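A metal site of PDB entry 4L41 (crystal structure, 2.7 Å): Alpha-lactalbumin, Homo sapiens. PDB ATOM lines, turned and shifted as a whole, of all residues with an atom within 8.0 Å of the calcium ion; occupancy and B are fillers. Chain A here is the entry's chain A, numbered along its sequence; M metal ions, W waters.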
ATOM      1  N   THR A  39      -9.355   8.932  24.212  1.00  0.00           N
ATOM      2  CA  THR A  39     -10.022   8.943  22.910  1.00  0.00           C
ATOM      3  C   THR A  39     -11.254   8.052  22.897  1.00  0.00           C
ATOM      4  O   THR A  39     -12.059   8.110  21.971  1.00  0.00           O
ATOM      5  CB  THR A  39      -9.067   8.491  21.802  1.00  0.00           C
ATOM      6  OG1 THR A  39      -8.469   7.239  22.172  1.00  0.00           O
ATOM      7  CG2 THR A  39      -7.993   9.514  21.591  1.00  0.00           C
ATOM      8  N   ILE A  76     -20.321  12.864   9.922  1.00  0.00           N
ATOM      9  CA  ILE A  76     -19.546  11.725  10.415  1.00  0.00           C
ATOM     10  C   ILE A  76     -20.323  10.829  11.389  1.00  0.00           C
ATOM     11  O   ILE A  76     -21.251  11.279  12.069  1.00  0.00           O
ATOM     12  CB  ILE A  76     -18.250  12.219  11.084  1.00  0.00           C
ATOM     13  CG1 ILE A  76     -17.177  11.126  11.091  1.00  0.00           C
ATOM     14  CG2 ILE A  76     -18.533  12.719  12.487  1.00  0.00           C
ATOM     15  CD1 ILE A  76     -15.789  11.660  11.337  1.00  0.00           C
ATOM     16  N   SER A  77     -19.947   9.555  11.438  1.00  0.00           N
ATOM     17  CA  SER A  77     -20.459   8.630  12.436  1.00  0.00           C
ATOM     18  C   SER A  77     -19.832   8.967  13.778  1.00  0.00           C
ATOM     19  O   SER A  77     -18.644   9.309  13.845  1.00  0.00           O
ATOM     20  CB  SER A  77     -20.118   7.193  12.066  1.00  0.00           C
ATOM     21  OG  SER A  77     -20.598   6.873  10.774  1.00  0.00           O
ATOM     22  N   CYS A  78     -20.599   8.864  14.836  1.00  0.00           N
ATOM     23  CA  CYS A  78     -20.144   9.219  16.153  1.00  0.00           C
ATOM     24  C   CYS A  78     -19.020   8.338  16.587  1.00  0.00           C
ATOM     25  O   CYS A  78     -18.253   8.671  17.416  1.00  0.00           O
ATOM     26  CB  CYS A  78     -21.317   9.211  17.129  1.00  0.00           C
ATOM     27  SG  CYS A  78     -22.091  10.711  17.217  1.00  0.00           S
ATOM     28  N   ASP A  79     -18.903   7.210  15.950  1.00  0.00           N
ATOM     29  CA  ASP A  79     -17.939   6.224  16.307  1.00  0.00           C
ATOM     30  C   ASP A  79     -16.553   6.487  15.805  1.00  0.00           C
ATOM     31  O   ASP A  79     -15.647   5.820  16.217  1.00  0.00           O
ATOM     32  CB  ASP A  79     -18.376   4.901  15.764  1.00  0.00           C
ATOM     33  CG  ASP A  79     -19.376   4.240  16.604  1.00  0.00           C
ATOM     34  OD1 ASP A  79     -19.547   4.585  17.757  1.00  0.00           O
ATOM     35  OD2 ASP A  79     -19.998   3.303  16.102  1.00  0.00           O
ATOM     36  N   LYS A  80     -16.380   7.438  14.943  1.00  0.00           N
ATOM     37  CA  LYS A  80     -15.069   7.730  14.547  1.00  0.00           C
ATOM     38  C   LYS A  80     -14.379   8.646  15.552  1.00  0.00           C
ATOM     39  O   LYS A  80     -13.269   9.134  15.348  1.00  0.00           O
ATOM     40  CB  LYS A  80     -15.175   8.575  13.333  1.00  0.00           C
ATOM     41  CG  LYS A  80     -15.521   7.843  12.144  1.00  0.00           C
ATOM     42  CD  LYS A  80     -14.343   7.023  11.710  1.00  0.00           C
ATOM     43  CE  LYS A  80     -14.618   6.427  10.394  1.00  0.00           C
ATOM     44  NZ  LYS A  80     -13.819   5.290  10.059  1.00  0.00           N
ATOM     45  N   PHE A  81     -15.050   8.899  16.647  1.00  0.00           N
ATOM     46  CA  PHE A  81     -14.541   9.723  17.669  1.00  0.00           C
ATOM     47  C   PHE A  81     -14.104   8.861  18.841  1.00  0.00           C
ATOM     48  O   PHE A  81     -13.942   9.300  19.918  1.00  0.00           O
ATOM     49  CB  PHE A  81     -15.617  10.686  18.066  1.00  0.00           C
ATOM     50  CG  PHE A  81     -15.940  11.701  17.032  1.00  0.00           C
ATOM     51  CD1 PHE A  81     -15.037  12.041  16.074  1.00  0.00           C
ATOM     52  CD2 PHE A  81     -17.158  12.318  17.033  1.00  0.00           C
ATOM     53  CE1 PHE A  81     -15.337  12.954  15.156  1.00  0.00           C
ATOM     54  CE2 PHE A  81     -17.438  13.225  16.108  1.00  0.00           C
ATOM     55  CZ  PHE A  81     -16.520  13.544  15.185  1.00  0.00           C
ATOM     56  N   LEU A  82     -13.879   7.595  18.565  1.00  0.00           N
ATOM     57  CA  LEU A  82     -13.455   6.606  19.496  1.00  0.00           C
ATOM     58  C   LEU A  82     -12.248   5.854  19.052  1.00  0.00           C
ATOM     59  O   LEU A  82     -11.766   5.084  19.768  1.00  0.00           O
ATOM     60  CB  LEU A  82     -14.591   5.674  19.800  1.00  0.00           C
ATOM     61  CG  LEU A  82     -15.904   6.287  20.202  1.00  0.00           C
ATOM     62  CD1 LEU A  82     -16.901   5.256  20.245  1.00  0.00           C
ATOM     63  CD2 LEU A  82     -15.739   6.847  21.511  1.00  0.00           C
ATOM     64  N   ASP A  83     -11.763   6.105  17.857  1.00  0.00           N
ATOM     65  CA  ASP A  83     -10.523   5.532  17.356  1.00  0.00           C
ATOM     66  C   ASP A  83      -9.303   6.196  17.986  1.00  0.00           C
ATOM     67  O   ASP A  83      -9.427   6.891  18.992  1.00  0.00           O
ATOM     68  CB  ASP A  83     -10.463   5.670  15.833  1.00  0.00           C
ATOM     69  CG  ASP A  83     -10.615   7.109  15.372  1.00  0.00           C
ATOM     70  OD1 ASP A  83     -11.127   7.939  16.145  1.00  0.00           O
ATOM     71  OD2 ASP A  83     -10.224   7.395  14.218  1.00  0.00           O
ATOM     72  N   ASP A  84      -8.138   5.994  17.395  1.00  0.00           N
ATOM     73  CA  ASP A  84      -6.903   6.538  17.946  1.00  0.00           C
ATOM     74  C   ASP A  84      -6.366   7.686  17.096  1.00  0.00           C
ATOM     75  O   ASP A  84      -5.245   8.154  17.305  1.00  0.00           O
ATOM     76  CB  ASP A  84      -5.859   5.441  18.100  1.00  0.00           C
ATOM     77  CG  ASP A  84      -6.323   4.316  18.994  1.00  0.00           C
ATOM     78  OD1 ASP A  84      -7.248   4.540  19.808  1.00  0.00           O
ATOM     79  OD2 ASP A  84      -5.773   3.191  18.892  1.00  0.00           O
ATOM     80  N   ASP A  85      -7.174   8.132  16.152  1.00  0.00           N
ATOM     81  CA  ASP A  85      -6.825   9.274  15.323  1.00  0.00           C
ATOM     82  C   ASP A  85      -7.798  10.406  15.652  1.00  0.00           C
ATOM     83  O   ASP A  85      -9.011  10.232  15.585  1.00  0.00           O
ATOM     84  CB  ASP A  85      -6.923   8.924  13.841  1.00  0.00           C
ATOM     85  CG  ASP A  85      -6.243   9.935  12.947  1.00  0.00           C
ATOM     86  OD1 ASP A  85      -5.996  11.066  13.412  1.00  0.00           O
ATOM     87  OD2 ASP A  85      -5.947   9.605  11.777  1.00  0.00           O
ATOM     88  N   ILE A  86      -7.262  11.564  16.021  1.00  0.00           N
ATOM     89  CA  ILE A  86      -8.095  12.713  16.349  1.00  0.00           C
ATOM     90  C   ILE A  86      -8.101  13.754  15.235  1.00  0.00           C
ATOM     91  O   ILE A  86      -8.400  14.924  15.463  1.00  0.00           O
ATOM     92  CB  ILE A  86      -7.668  13.363  17.683  1.00  0.00           C
ATOM     93  CG1 ILE A  86      -6.207  13.819  17.608  1.00  0.00           C
ATOM     94  CG2 ILE A  86      -7.854  12.399  18.844  1.00  0.00           C
ATOM     95  CD1 ILE A  86      -5.744  14.569  18.845  1.00  0.00           C
ATOM     96  N   THR A  87      -7.763  13.321  14.025  1.00  0.00           N
ATOM     97  CA  THR A  87      -7.757  14.216  12.862  1.00  0.00           C
ATOM     98  C   THR A  87      -9.150  14.755  12.589  1.00  0.00           C
ATOM     99  O   THR A  87      -9.333  15.972  12.431  1.00  0.00           O
ATOM    100  CB  THR A  87      -7.239  13.496  11.604  1.00  0.00           C
ATOM    101  OG1 THR A  87      -5.965  12.892  11.867  1.00  0.00           O
ATOM    102  CG2 THR A  87      -7.091  14.481  10.458  1.00  0.00           C
ATOM    103  N   ASP A  88     -10.135  13.862  12.545  1.00  0.00           N
ATOM    104  CA  ASP A  88     -11.510  14.256  12.274  1.00  0.00           C
ATOM    105  C   ASP A  88     -12.259  14.712  13.527  1.00  0.00           C
ATOM    106  O   ASP A  88     -13.312  15.345  13.421  1.00  0.00           O
ATOM    107  CB  ASP A  88     -12.282  13.122  11.589  1.00  0.00           C
ATOM    108  CG  ASP A  88     -12.056  11.787  12.241  1.00  0.00           C
ATOM    109  OD1 ASP A  88     -11.497  11.746  13.360  1.00  0.00           O
ATOM    110  OD2 ASP A  88     -12.451  10.759  11.644  1.00  0.00           O
ATOM    111  N   ASP A  89     -11.725  14.382  14.703  1.00  0.00           N
ATOM    112  CA  ASP A  89     -12.260  14.917  15.948  1.00  0.00           C
ATOM    113  C   ASP A  89     -12.017  16.420  15.985  1.00  0.00           C
ATOM    114  O   ASP A  89     -12.891  17.203  16.351  1.00  0.00           O
ATOM    115  CB  ASP A  89     -11.567  14.264  17.147  1.00  0.00           C
ATOM    116  CG  ASP A  89     -12.041  12.853  17.406  1.00  0.00           C
ATOM    117  OD1 ASP A  89     -11.584  11.932  16.709  1.00  0.00           O
ATOM    118  OD2 ASP A  89     -12.863  12.662  18.333  1.00  0.00           O
ATOM    119  N   ILE A  90     -10.814  16.812  15.588  1.00  0.00           N
ATOM    120  CA  ILE A  90     -10.418  18.206  15.528  1.00  0.00           C
ATOM    121  C   ILE A  90     -11.256  19.001  14.531  1.00  0.00           C
ATOM    122  O   ILE A  90     -11.642  20.142  14.791  1.00  0.00           O
ATOM    123  CB  ILE A  90      -8.897  18.330  15.211  1.00  0.00           C
ATOM    124  CG1 ILE A  90      -8.072  17.868  16.412  1.00  0.00           C
ATOM    125  CG2 ILE A  90      -8.530  19.745  14.823  1.00  0.00           C
ATOM    126  CD1 ILE A  90      -6.619  17.590  16.082  1.00  0.00           C
HETATM  127 CA    CA M   1     -11.207  10.028  15.095  1.00  0.00          CA
HETATM  128  O   HOH W   1     -10.708   9.984  17.698  1.00  0.00           O
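Within 4 Å of the calcium ion: Lys 80, Asp 83, Asp 85, Asp 88 and Asp 89.
The nearest printed residue that does not touch the calcium ion is Phe 81 (4.2 Å).
N of Thr 87 is in hydrogen-bond range of OD1 of Asp 85 (2.9 Å).
The side-chain hydroxyl (OG1) of Thr 39 lies close to the backbone carbonyl oxygen (O) of Asp 83.
The calcium ion is bound by the backbone carbonyl oxygen of Asp 85 (2.3 Å), the backbone carbonyl oxygen of Lys 80 (2.3 Å), the side-chain carboxylate of Asp 83 (2.3 Å), the side-chain carboxylate of Asp 88 (2.5 Å), the side-chain carboxylate of Asp 89 (2.5 Å) and water W1 (2.7 Å).
The calcium ion has six donor atoms within binding distance.
Slightly farther from the calcium ion lies OD2 of Asp 83 (2.9 Å).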
